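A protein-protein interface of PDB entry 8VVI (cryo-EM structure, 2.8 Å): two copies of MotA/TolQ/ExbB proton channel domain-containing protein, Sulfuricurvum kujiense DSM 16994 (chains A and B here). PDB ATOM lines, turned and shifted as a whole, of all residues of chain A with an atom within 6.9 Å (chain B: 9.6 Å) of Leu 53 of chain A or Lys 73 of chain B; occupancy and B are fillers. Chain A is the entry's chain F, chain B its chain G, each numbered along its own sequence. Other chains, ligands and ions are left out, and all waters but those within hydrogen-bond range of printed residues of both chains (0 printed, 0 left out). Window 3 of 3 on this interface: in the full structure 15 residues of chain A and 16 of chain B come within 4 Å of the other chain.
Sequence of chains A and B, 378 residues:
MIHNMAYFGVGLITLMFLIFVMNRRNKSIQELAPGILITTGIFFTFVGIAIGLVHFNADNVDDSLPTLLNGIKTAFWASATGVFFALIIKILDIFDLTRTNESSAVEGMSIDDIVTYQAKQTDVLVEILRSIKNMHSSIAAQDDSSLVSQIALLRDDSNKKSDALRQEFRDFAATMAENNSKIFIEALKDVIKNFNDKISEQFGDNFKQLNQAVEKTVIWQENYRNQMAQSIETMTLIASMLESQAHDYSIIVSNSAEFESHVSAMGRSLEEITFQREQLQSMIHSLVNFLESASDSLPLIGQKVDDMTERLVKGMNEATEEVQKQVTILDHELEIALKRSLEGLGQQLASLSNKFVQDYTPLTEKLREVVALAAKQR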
ATOM      1  N   VAL A  47      33.697   0.927  21.675  1.00  0.00           N
ATOM      2  CA  VAL A  47      33.565  -0.516  21.489  1.00  0.00           C
ATOM      3  C   VAL A  47      34.125  -1.256  22.697  1.00  0.00           C
ATOM      4  O   VAL A  47      33.554  -2.256  23.149  1.00  0.00           O
ATOM      5  CB  VAL A  47      34.253  -0.949  20.180  1.00  0.00           C
ATOM      6  CG1 VAL A  47      34.413  -2.460  20.131  1.00  0.00           C
ATOM      7  CG2 VAL A  47      33.459  -0.461  18.982  1.00  0.00           C
ATOM      8  N   GLY A  48      35.243  -0.771  23.244  1.00  0.00           N
ATOM      9  CA  GLY A  48      35.820  -1.410  24.415  1.00  0.00           C
ATOM     10  C   GLY A  48      34.887  -1.406  25.611  1.00  0.00           C
ATOM     11  O   GLY A  48      34.740  -2.419  26.297  1.00  0.00           O
ATOM     12  N   ILE A  49      34.244  -0.267  25.880  1.00  0.00           N
ATOM     13  CA  ILE A  49      33.256  -0.218  26.952  1.00  0.00           C
ATOM     14  C   ILE A  49      32.065  -1.106  26.618  1.00  0.00           C
ATOM     15  O   ILE A  49      31.521  -1.793  27.489  1.00  0.00           O
ATOM     16  CB  ILE A  49      32.816   1.232  27.222  1.00  0.00           C
ATOM     17  CG1 ILE A  49      34.003   2.185  27.115  1.00  0.00           C
ATOM     18  CG2 ILE A  49      32.190   1.344  28.598  1.00  0.00           C
ATOM     19  CD1 ILE A  49      33.619   3.641  27.069  1.00  0.00           C
ATOM     20  N   ALA A  50      31.636  -1.097  25.354  1.00  0.00           N
ATOM     21  CA  ALA A  50      30.492  -1.908  24.952  1.00  0.00           C
ATOM     22  C   ALA A  50      30.783  -3.397  25.102  1.00  0.00           C
ATOM     23  O   ALA A  50      29.945  -4.150  25.612  1.00  0.00           O
ATOM     24  CB  ALA A  50      30.101  -1.578  23.512  1.00  0.00           C
ATOM     25  N   ILE A  51      31.964  -3.842  24.668  1.00  0.00           N
ATOM     26  CA  ILE A  51      32.307  -5.256  24.797  1.00  0.00           C
ATOM     27  C   ILE A  51      32.855  -5.589  26.177  1.00  0.00           C
ATOM     28  O   ILE A  51      32.863  -6.765  26.563  1.00  0.00           O
ATOM     29  CB  ILE A  51      33.314  -5.688  23.716  1.00  0.00           C
ATOM     30  CG1 ILE A  51      34.698  -5.099  23.998  1.00  0.00           C
ATOM     31  CG2 ILE A  51      32.816  -5.295  22.333  1.00  0.00           C
ATOM     32  CD1 ILE A  51      35.805  -5.713  23.172  1.00  0.00           C
ATOM     33  N   GLY A  52      33.322  -4.592  26.932  1.00  0.00           N
ATOM     34  CA  GLY A  52      33.766  -4.841  28.291  1.00  0.00           C
ATOM     35  C   GLY A  52      32.647  -4.954  29.302  1.00  0.00           C
ATOM     36  O   GLY A  52      32.864  -5.491  30.393  1.00  0.00           O
ATOM     37  N   LEU A  53      31.456  -4.465  28.964  1.00  0.00           N
ATOM     38  CA  LEU A  53      30.305  -4.516  29.852  1.00  0.00           C
ATOM     39  C   LEU A  53      29.189  -5.411  29.330  1.00  0.00           C
ATOM     40  O   LEU A  53      28.175  -5.570  30.016  1.00  0.00           O
ATOM     41  CB  LEU A  53      29.760  -3.103  30.091  1.00  0.00           C
ATOM     42  CG  LEU A  53      30.596  -2.169  30.967  1.00  0.00           C
ATOM     43  CD1 LEU A  53      30.041  -0.757  30.918  1.00  0.00           C
ATOM     44  CD2 LEU A  53      30.651  -2.676  32.400  1.00  0.00           C
ATOM     45  N   VAL A  54      29.350  -6.000  28.143  1.00  0.00           N
ATOM     46  CA  VAL A  54      28.280  -6.810  27.568  1.00  0.00           C
ATOM     47  C   VAL A  54      28.036  -8.064  28.399  1.00  0.00           C
ATOM     48  O   VAL A  54      26.892  -8.514  28.535  1.00  0.00           O
ATOM     49  CB  VAL A  54      28.595  -7.146  26.095  1.00  0.00           C
ATOM     50  CG1 VAL A  54      29.869  -7.971  25.982  1.00  0.00           C
ATOM     51  CG2 VAL A  54      27.424  -7.867  25.447  1.00  0.00           C
ATOM     52  N   HIS A  55      29.089  -8.643  28.976  1.00  0.00           N
ATOM     53  CA  HIS A  55      28.977  -9.849  29.786  1.00  0.00           C
ATOM     54  C   HIS A  55      29.103  -9.556  31.276  1.00  0.00           C
ATOM     55  O   HIS A  55      29.400 -10.462  32.060  1.00  0.00           O
ATOM     56  CB  HIS A  55      30.022 -10.877  29.354  1.00  0.00           C
ATOM     57  CG  HIS A  55      29.774 -11.452  27.995  1.00  0.00           C
ATOM     58  ND1 HIS A  55      28.507 -11.658  27.494  1.00  0.00           N
ATOM     59  CD2 HIS A  55      30.632 -11.862  27.030  1.00  0.00           C
ATOM     60  CE1 HIS A  55      28.594 -12.172  26.280  1.00  0.00           C
ATOM     61  NE2 HIS A  55      29.872 -12.305  25.974  1.00  0.00           N
ATOM     62  N   PHE A  56      28.888  -8.307  31.681  1.00  0.00           N
ATOM     63  CA  PHE A  56      28.956  -7.957  33.092  1.00  0.00           C
ATOM     64  C   PHE A  56      27.741  -8.510  33.828  1.00  0.00           C
ATOM     65  O   PHE A  56      26.603  -8.360  33.373  1.00  0.00           O
ATOM     66  CB  PHE A  56      29.034  -6.441  33.263  1.00  0.00           C
ATOM     67  CG  PHE A  56      29.183  -5.999  34.691  1.00  0.00           C
ATOM     68  CD1 PHE A  56      30.430  -5.966  35.292  1.00  0.00           C
ATOM     69  CD2 PHE A  56      28.077  -5.616  35.433  1.00  0.00           C
ATOM     70  CE1 PHE A  56      30.570  -5.560  36.605  1.00  0.00           C
ATOM     71  CE2 PHE A  56      28.212  -5.211  36.745  1.00  0.00           C
ATOM     72  CZ  PHE A  56      29.460  -5.182  37.332  1.00  0.00           C
ATOM     73  N   ASN A  57      27.987  -9.151  34.967  1.00  0.00           N
ATOM     74  CA  ASN A  57      26.936  -9.712  35.803  1.00  0.00           C
ATOM     75  C   ASN A  57      26.984  -9.047  37.171  1.00  0.00           C
ATOM     76  O   ASN A  57      28.042  -9.003  37.806  1.00  0.00           O
ATOM     77  CB  ASN A  57      27.090 -11.229  35.941  1.00  0.00           C
ATOM     78  CG  ASN A  57      25.781 -11.921  36.257  1.00  0.00           C
ATOM     79  OD1 ASN A  57      24.720 -11.296  36.261  1.00  0.00           O
ATOM     80  ND2 ASN A  57      25.848 -13.219  36.528  1.00  0.00           N
ATOM     81  N   ALA A  58      25.838  -8.524  37.614  1.00  0.00           N
ATOM     82  CA  ALA A  58      25.778  -7.891  38.928  1.00  0.00           C
ATOM     83  C   ALA A  58      26.034  -8.902  40.038  1.00  0.00           C
ATOM     84  O   ALA A  58      26.733  -8.602  41.013  1.00  0.00           O
ATOM     85  CB  ALA A  58      24.424  -7.210  39.121  1.00  0.00           C
ATOM     86  N   THR A  67      36.693 -10.049  31.025  1.00  0.00           N
ATOM     87  CA  THR A  67      35.979  -9.450  29.903  1.00  0.00           C
ATOM     88  C   THR A  67      36.098  -7.931  29.924  1.00  0.00           C
ATOM     89  O   THR A  67      36.251  -7.300  28.873  1.00  0.00           O
ATOM     90  CB  THR A  67      34.510  -9.871  29.930  1.00  0.00           C
ATOM     91  OG1 THR A  67      34.418 -11.272  30.218  1.00  0.00           O
ATOM     92  CG2 THR A  67      33.850  -9.594  28.587  1.00  0.00           C
ATOM     93  N   LEU A  68      36.031  -7.328  31.113  1.00  0.00           N
ATOM     94  CA  LEU A  68      36.166  -5.881  31.219  1.00  0.00           C
ATOM     95  C   LEU A  68      37.606  -5.437  30.992  1.00  0.00           C
ATOM     96  O   LEU A  68      37.840  -4.339  30.476  1.00  0.00           O
ATOM     97  CB  LEU A  68      35.659  -5.410  32.582  1.00  0.00           C
ATOM     98  CG  LEU A  68      35.654  -3.909  32.867  1.00  0.00           C
ATOM     99  CD1 LEU A  68      34.729  -3.184  31.906  1.00  0.00           C
ATOM    100  CD2 LEU A  68      35.234  -3.652  34.303  1.00  0.00           C
ATOM    101  N   GLY A  71      38.096  -4.952  27.299  1.00  0.00           N
ATOM    102  CA  GLY A  71      37.643  -3.674  26.776  1.00  0.00           C
ATOM    103  C   GLY A  71      38.608  -2.539  27.059  1.00  0.00           C
ATOM    104  O   GLY A  71      38.840  -1.684  26.201  1.00  0.00           O
ATOM    105  N   ILE B   2      16.497   1.080  29.834  1.00  0.00           N
ATOM    106  CA  ILE B   2      17.782   1.439  29.238  1.00  0.00           C
ATOM    107  C   ILE B   2      18.114   0.507  28.080  1.00  0.00           C
ATOM    108  O   ILE B   2      18.631   0.940  27.043  1.00  0.00           O
ATOM    109  CB  ILE B   2      18.890   1.432  30.306  1.00  0.00           C
ATOM    110  CG1 ILE B   2      18.364   2.002  31.623  1.00  0.00           C
ATOM    111  CG2 ILE B   2      20.093   2.228  29.824  1.00  0.00           C
ATOM    112  CD1 ILE B   2      19.343   1.894  32.770  1.00  0.00           C
ATOM    113  N   HIS B   3      17.840  -0.790  28.245  1.00  0.00           N
ATOM    114  CA  HIS B   3      18.100  -1.742  27.171  1.00  0.00           C
ATOM    115  C   HIS B   3      17.249  -1.441  25.942  1.00  0.00           C
ATOM    116  O   HIS B   3      17.742  -1.503  24.810  1.00  0.00           O
ATOM    117  CB  HIS B   3      17.848  -3.167  27.660  1.00  0.00           C
ATOM    118  CG  HIS B   3      18.791  -3.614  28.733  1.00  0.00           C
ATOM    119  ND1 HIS B   3      20.093  -3.984  28.473  1.00  0.00           N
ATOM    120  CD2 HIS B   3      18.622  -3.751  30.069  1.00  0.00           C
ATOM    121  CE1 HIS B   3      20.685  -4.329  29.602  1.00  0.00           C
ATOM    122  NE2 HIS B   3      19.814  -4.197  30.586  1.00  0.00           N
ATOM    123  N   MET B   5      15.864   1.461  24.968  1.00  0.00           N
ATOM    124  CA  MET B   5      16.257   2.693  24.296  1.00  0.00           C
ATOM    125  C   MET B   5      17.620   2.577  23.629  1.00  0.00           C
ATOM    126  O   MET B   5      17.961   3.421  22.794  1.00  0.00           O
ATOM    127  CB  MET B   5      16.231   3.867  25.284  1.00  0.00           C
ATOM    128  CG  MET B   5      17.175   3.754  26.478  1.00  0.00           C
ATOM    129  SD  MET B   5      18.901   4.160  26.144  1.00  0.00           S
ATOM    130  CE  MET B   5      18.789   5.932  25.913  1.00  0.00           C
ATOM    131  N   ALA B   6      18.407   1.557  23.982  1.00  0.00           N
ATOM    132  CA  ALA B   6      19.663   1.317  23.281  1.00  0.00           C
ATOM    133  C   ALA B   6      19.418   0.934  21.826  1.00  0.00           C
ATOM    134  O   ALA B   6      20.099   1.434  20.925  1.00  0.00           O
ATOM    135  CB  ALA B   6      20.467   0.232  23.994  1.00  0.00           C
ATOM    136  N   VAL B  10      20.499   3.197  18.723  1.00  0.00           N
ATOM    137  CA  VAL B  10      21.263   2.618  17.623  1.00  0.00           C
ATOM    138  C   VAL B  10      20.448   2.638  16.336  1.00  0.00           C
ATOM    139  O   VAL B  10      20.955   3.001  15.269  1.00  0.00           O
ATOM    140  CB  VAL B  10      21.721   1.194  17.984  1.00  0.00           C
ATOM    141  CG1 VAL B  10      22.292   0.490  16.764  1.00  0.00           C
ATOM    142  CG2 VAL B  10      22.747   1.235  19.103  1.00  0.00           C
ATOM    143  N   THR B  45      23.818   7.865  24.910  1.00  0.00           N
ATOM    144  CA  THR B  45      24.665   7.351  25.981  1.00  0.00           C
ATOM    145  C   THR B  45      24.410   8.097  27.285  1.00  0.00           C
ATOM    146  O   THR B  45      24.324   7.483  28.354  1.00  0.00           O
ATOM    147  CB  THR B  45      26.137   7.454  25.580  1.00  0.00           C
ATOM    148  OG1 THR B  45      26.410   6.518  24.530  1.00  0.00           O
ATOM    149  CG2 THR B  45      27.043   7.152  26.763  1.00  0.00           C
ATOM    150  N   GLY B  48      21.069   7.036  28.672  1.00  0.00           N
ATOM    151  CA  GLY B  48      21.168   5.703  29.239  1.00  0.00           C
ATOM    152  C   GLY B  48      21.819   5.683  30.607  1.00  0.00           C
ATOM    153  O   GLY B  48      21.444   4.881  31.466  1.00  0.00           O
ATOM    154  N   ILE B  49      22.800   6.556  30.830  1.00  0.00           N
ATOM    155  CA  ILE B  49      23.429   6.647  32.142  1.00  0.00           C
ATOM    156  C   ILE B  49      22.579   7.485  33.090  1.00  0.00           C
ATOM    157  O   ILE B  49      22.509   7.202  34.291  1.00  0.00           O
ATOM    158  CB  ILE B  49      24.857   7.205  32.004  1.00  0.00           C
ATOM    159  CG1 ILE B  49      25.672   6.327  31.051  1.00  0.00           C
ATOM    160  CG2 ILE B  49      25.535   7.292  33.364  1.00  0.00           C
ATOM    161  CD1 ILE B  49      27.162   6.564  31.108  1.00  0.00           C
ATOM    162  N   GLY B  52      19.930   5.247  34.388  1.00  0.00           N
ATOM    163  CA  GLY B  52      20.506   4.337  35.359  1.00  0.00           C
ATOM    164  C   GLY B  52      21.002   5.000  36.627  1.00  0.00           C
ATOM    165  O   GLY B  52      21.257   4.297  37.610  1.00  0.00           O
ATOM    166  N   LEU B  65      25.874  -0.026  42.923  1.00  0.00           N
ATOM    167  CA  LEU B  65      26.850   0.185  41.854  1.00  0.00           C
ATOM    168  C   LEU B  65      26.897  -0.989  40.881  1.00  0.00           C
ATOM    169  O   LEU B  65      26.903  -0.748  39.662  1.00  0.00           O
ATOM    170  CB  LEU B  65      28.224   0.498  42.455  1.00  0.00           C
ATOM    171  CG  LEU B  65      29.370   0.710  41.465  1.00  0.00           C
ATOM    172  CD1 LEU B  65      28.961   1.649  40.343  1.00  0.00           C
ATOM    173  CD2 LEU B  65      30.603   1.239  42.182  1.00  0.00           C
ATOM    174  N   PRO B  66      26.942  -2.255  41.319  1.00  0.00           N
ATOM    175  CA  PRO B  66      26.808  -3.350  40.343  1.00  0.00           C
ATOM    176  C   PRO B  66      25.508  -3.296  39.564  1.00  0.00           C
ATOM    177  O   PRO B  66      25.480  -3.692  38.393  1.00  0.00           O
ATOM    178  CB  PRO B  66      26.896  -4.610  41.215  1.00  0.00           C
ATOM    179  CG  PRO B  66      27.674  -4.188  42.400  1.00  0.00           C
ATOM    180  CD  PRO B  66      27.269  -2.769  42.663  1.00  0.00           C
ATOM    181  N   THR B  67      24.424  -2.821  40.181  1.00  0.00           N
ATOM    182  CA  THR B  67      23.189  -2.598  39.437  1.00  0.00           C
ATOM    183  C   THR B  67      23.347  -1.452  38.446  1.00  0.00           C
ATOM    184  O   THR B  67      22.801  -1.502  37.338  1.00  0.00           O
ATOM    185  CB  THR B  67      22.036  -2.315  40.400  1.00  0.00           C
ATOM    186  OG1 THR B  67      22.073  -3.255  41.481  1.00  0.00           O
ATOM    187  CG2 THR B  67      20.701  -2.431  39.682  1.00  0.00           C
ATOM    188  N   LEU B  68      24.083  -0.408  38.832  1.00  0.00           N
ATOM    189  CA  LEU B  68      24.318   0.714  37.927  1.00  0.00           C
ATOM    190  C   LEU B  68      25.122   0.278  36.709  1.00  0.00           C
ATOM    191  O   LEU B  68      24.803   0.652  35.575  1.00  0.00           O
ATOM    192  CB  LEU B  68      25.030   1.845  38.670  1.00  0.00           C
ATOM    193  CG  LEU B  68      25.586   2.987  37.820  1.00  0.00           C
ATOM    194  CD1 LEU B  68      24.462   3.832  37.250  1.00  0.00           C
ATOM    195  CD2 LEU B  68      26.537   3.843  38.637  1.00  0.00           C
ATOM    196  N   LEU B  69      26.171  -0.521  36.923  1.00  0.00           N
ATOM    197  CA  LEU B  69      26.972  -1.001  35.802  1.00  0.00           C
ATOM    198  C   LEU B  69      26.191  -1.976  34.931  1.00  0.00           C
ATOM    199  O   LEU B  69      26.375  -1.995  33.709  1.00  0.00           O
ATOM    200  CB  LEU B  69      28.254  -1.656  36.314  1.00  0.00           C
ATOM    201  CG  LEU B  69      29.121  -0.811  37.249  1.00  0.00           C
ATOM    202  CD1 LEU B  69      30.209  -1.658  37.885  1.00  0.00           C
ATOM    203  CD2 LEU B  69      29.722   0.369  36.504  1.00  0.00           C
ATOM    204  N   ASN B  70      25.320  -2.786  35.535  1.00  0.00           N
ATOM    205  CA  ASN B  70      24.510  -3.721  34.764  1.00  0.00           C
ATOM    206  C   ASN B  70      23.419  -3.020  33.966  1.00  0.00           C
ATOM    207  O   ASN B  70      22.864  -3.619  33.039  1.00  0.00           O
ATOM    208  CB  ASN B  70      23.887  -4.765  35.692  1.00  0.00           C
ATOM    209  CG  ASN B  70      23.329  -5.956  34.939  1.00  0.00           C
ATOM    210  OD1 ASN B  70      24.056  -6.893  34.612  1.00  0.00           O
ATOM    211  ND2 ASN B  70      22.032  -5.926  34.659  1.00  0.00           N
ATOM    212  N   GLY B  71      23.094  -1.775  34.303  1.00  0.00           N
ATOM    213  CA  GLY B  71      22.057  -1.058  33.590  1.00  0.00           C
ATOM    214  C   GLY B  71      22.582  -0.184  32.471  1.00  0.00           C
ATOM    215  O   GLY B  71      21.852   0.133  31.529  1.00  0.00           O
ATOM    216  N   ILE B  72      23.853   0.207  32.558  1.00  0.00           N
ATOM    217  CA  ILE B  72      24.435   1.139  31.598  1.00  0.00           C
ATOM    218  C   ILE B  72      25.341   0.406  30.619  1.00  0.00           C
ATOM    219  O   ILE B  72      26.090   1.038  29.865  1.00  0.00           O
ATOM    220  CB  ILE B  72      25.208   2.260  32.318  1.00  0.00           C
ATOM    221  CG1 ILE B  72      26.453   1.691  33.000  1.00  0.00           C
ATOM    222  CG2 ILE B  72      24.311   2.967  33.322  1.00  0.00           C
ATOM    223  CD1 ILE B  72      27.473   2.736  33.376  1.00  0.00           C
ATOM    224  N   LYS B  73      25.282  -0.928  30.615  1.00  0.00           N
ATOM    225  CA  LYS B  73      26.141  -1.687  29.710  1.00  0.00           C
ATOM    226  C   LYS B  73      25.792  -1.429  28.249  1.00  0.00           C
ATOM    227  O   LYS B  73      26.684  -1.431  27.393  1.00  0.00           O
ATOM    228  CB  LYS B  73      26.065  -3.183  30.016  1.00  0.00           C
ATOM    229  CG  LYS B  73      24.709  -3.825  29.779  1.00  0.00           C
ATOM    230  CD  LYS B  73      24.748  -5.315  30.083  1.00  0.00           C
ATOM    231  CE  LYS B  73      24.818  -5.590  31.573  1.00  0.00           C
ATOM    232  NZ  LYS B  73      24.723  -7.047  31.868  1.00  0.00           N
ATOM    233  N   THR B  74      24.516  -1.207  27.944  1.00  0.00           N
ATOM    234  CA  THR B  74      24.071  -0.971  26.578  1.00  0.00           C
ATOM    235  C   THR B  74      24.019   0.507  26.216  1.00  0.00           C
ATOM    236  O   THR B  74      23.584   0.844  25.111  1.00  0.00           O
ATOM    237  CB  THR B  74      22.691  -1.600  26.358  1.00  0.00           C
ATOM    238  OG1 THR B  74      21.860  -1.342  27.495  1.00  0.00           O
ATOM    239  CG2 THR B  74      22.816  -3.102  26.160  1.00  0.00           C
ATOM    240  N   ALA B  75      24.450   1.394  27.116  1.00  0.00           N
ATOM    241  CA  ALA B  75      24.392   2.823  26.833  1.00  0.00           C
ATOM    242  C   ALA B  75      25.453   3.247  25.827  1.00  0.00           C
ATOM    243  O   ALA B  75      25.272   4.247  25.122  1.00  0.00           O
ATOM    244  CB  ALA B  75      24.542   3.620  28.127  1.00  0.00           C
ATOM    245  N   PHE B  76      26.555   2.508  25.738  1.00  0.00           N
ATOM    246  CA  PHE B  76      27.672   2.880  24.880  1.00  0.00           C
ATOM    247  C   PHE B  76      27.597   2.256  23.492  1.00  0.00           C
ATOM    248  O   PHE B  76      28.500   2.482  22.680  1.00  0.00           O
ATOM    249  CB  PHE B  76      28.994   2.501  25.551  1.00  0.00           C
ATOM    250  CG  PHE B  76      29.082   2.926  26.988  1.00  0.00           C
ATOM    251  CD1 PHE B  76      29.455   4.218  27.318  1.00  0.00           C
ATOM    252  CD2 PHE B  76      28.782   2.038  28.008  1.00  0.00           C
ATOM    253  CE1 PHE B  76      29.531   4.615  28.638  1.00  0.00           C
ATOM    254  CE2 PHE B  76      28.858   2.431  29.330  1.00  0.00           C
ATOM    255  CZ  PHE B  76      29.233   3.721  29.644  1.00  0.00           C
ATOM    256  N   TRP B  77      26.553   1.479  23.200  1.00  0.00           N
ATOM    257  CA  TRP B  77      26.380   0.967  21.845  1.00  0.00           C
ATOM    258  C   TRP B  77      25.961   2.070  20.883  1.00  0.00           C
ATOM    259  O   TRP B  77      26.343   2.043  19.708  1.00  0.00           O
ATOM    260  CB  TRP B  77      25.356  -0.166  21.834  1.00  0.00           C
ATOM    261  CG  TRP B  77      25.870  -1.452  22.408  1.00  0.00           C
ATOM    262  CD1 TRP B  77      25.424  -2.083  23.530  1.00  0.00           C
ATOM    263  CD2 TRP B  77      26.926  -2.267  21.884  1.00  0.00           C
ATOM    264  NE1 TRP B  77      26.135  -3.237  23.741  1.00  0.00           N
ATOM    265  CE2 TRP B  77      27.065  -3.374  22.743  1.00  0.00           C
ATOM    266  CE3 TRP B  77      27.768  -2.167  20.772  1.00  0.00           C
ATOM    267  CZ2 TRP B  77      28.010  -4.374  22.526  1.00  0.00           C
ATOM    268  CZ3 TRP B  77      28.706  -3.161  20.558  1.00  0.00           C
ATOM    269  CH2 TRP B  77      28.819  -4.250  21.431  1.00  0.00           C
ATOM    270  N   ALA B  78      25.175   3.038  21.357  1.00  0.00           N
ATOM    271  CA  ALA B  78      24.788   4.161  20.510  1.00  0.00           C
ATOM    272  C   ALA B  78      25.973   5.078  20.237  1.00  0.00           C
ATOM    273  O   ALA B  78      26.106   5.616  19.132  1.00  0.00           O
ATOM    274  CB  ALA B  78      23.643   4.937  21.157  1.00  0.00           C
ATOM    275  N   SER B  79      26.837   5.279  21.236  1.00  0.00           N
ATOM    276  CA  SER B  79      28.038   6.078  21.022  1.00  0.00           C
ATOM    277  C   SER B  79      28.955   5.430  19.995  1.00  0.00           C
ATOM    278  O   SER B  79      29.501   6.111  19.121  1.00  0.00           O
ATOM    279  CB  SER B  79      28.777   6.281  22.344  1.00  0.00           C
ATOM    280  OG  SER B  79      28.222   7.356  23.078  1.00  0.00           O
ATOM    281  N   ALA B  80      29.136   4.110  20.085  1.00  0.00           N
ATOM    282  CA  ALA B  80      29.941   3.405  19.094  1.00  0.00           C
ATOM    283  C   ALA B  80      29.295   3.471  17.716  1.00  0.00           C
ATOM    284  O   ALA B  80      29.989   3.615  16.704  1.00  0.00           O
ATOM    285  CB  ALA B  80      30.147   1.953  19.524  1.00  0.00           C
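O of Phe 56 of chain A lies close to OD1 of Asn 70 of chain B, at 3.2 Å.
The backbone carbonyl oxygen of Phe 56 of chain A is in hydrogen-bond range of the side-chain amino group of Lys 73 of chain B (2.7 Å).
NZ of Lys 73 of chain B is in hydrogen-bond range of OD1 of Asn 70 of chain B, at 2.8 Å.
Among the printed residues, merely in contact across the chains: Ile 49 of chain A with Phe 76 of chain B (3.5 Å), Ala 50 of chain A with Trp 77 of chain B (3.6 Å), Leu 53 of chain A with Lys 73 of chain B (3.2 Å), Leu 53 of chain A with Phe 76 of chain B (3.8 Å), Phe 56 of chain A with Pro 66 of chain B (3.5 Å), Phe 56 of chain A with Leu 69 of chain B (3.6 Å), Ala 58 of chain A with Pro 66 of chain B (3.7 Å) and Ala 58 of chain A with Asn 70 of chain B (3.9 Å).
Of chain B, only Lys 73 (3.2 Å) and Phe 76 (3.8 Å) come within 4 Å of Leu 53 of chain A.
Of chain A, only Leu 53 (3.2 Å) and Phe 56 (2.7 Å) come within 4 Å of Lys 73 of chain B.
Ala 50 of chain A touches one residue of chain B.
No residue of chain B comes within 4 Å of Gly 52 of chain A.
No residue of chain B comes within 4 Å of Val 54 of chain A.
Of the printed residues of chain B, Ala 58 of chain A touches Pro 66 (3.7 Å) and Asn 70 (3.9 Å).
Of the printed residues of chain A, Trp 77 of chain B touches Ala 50 (3.6 Å).
Of the printed residues of chain A, Leu 69 of chain B touches Phe 56 (3.6 Å).
Of the printed residues of chain A, Pro 66 of chain B touches Phe 56 (3.5 Å) and Ala 58 (3.7 Å).
Of the printed residues of chain B, Ile 49 of chain A touches Phe 76.
Ile 72 of chain B touches none of the printed residues of chain A.
His 3 of chain B touches none of the printed residues of chain A.
The nearest residue of chain B that does not touch Leu 53 of chain A is Ile 72 of chain B (4.5 Å).
Of the 15 printed residues of chain A, 5 touch a printed residue of chain B.
Hydrophobic or aromatic side chains of chain B that line the printed part of chain A: Leu 69, Phe 76 and Trp 77.
Positions printed for both chains: 48, 49, 52, 67, 68 and 71.
Of the 10 pairs that touch across the chains among the printed residues, none has its exchanged pair printed and touching as well.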
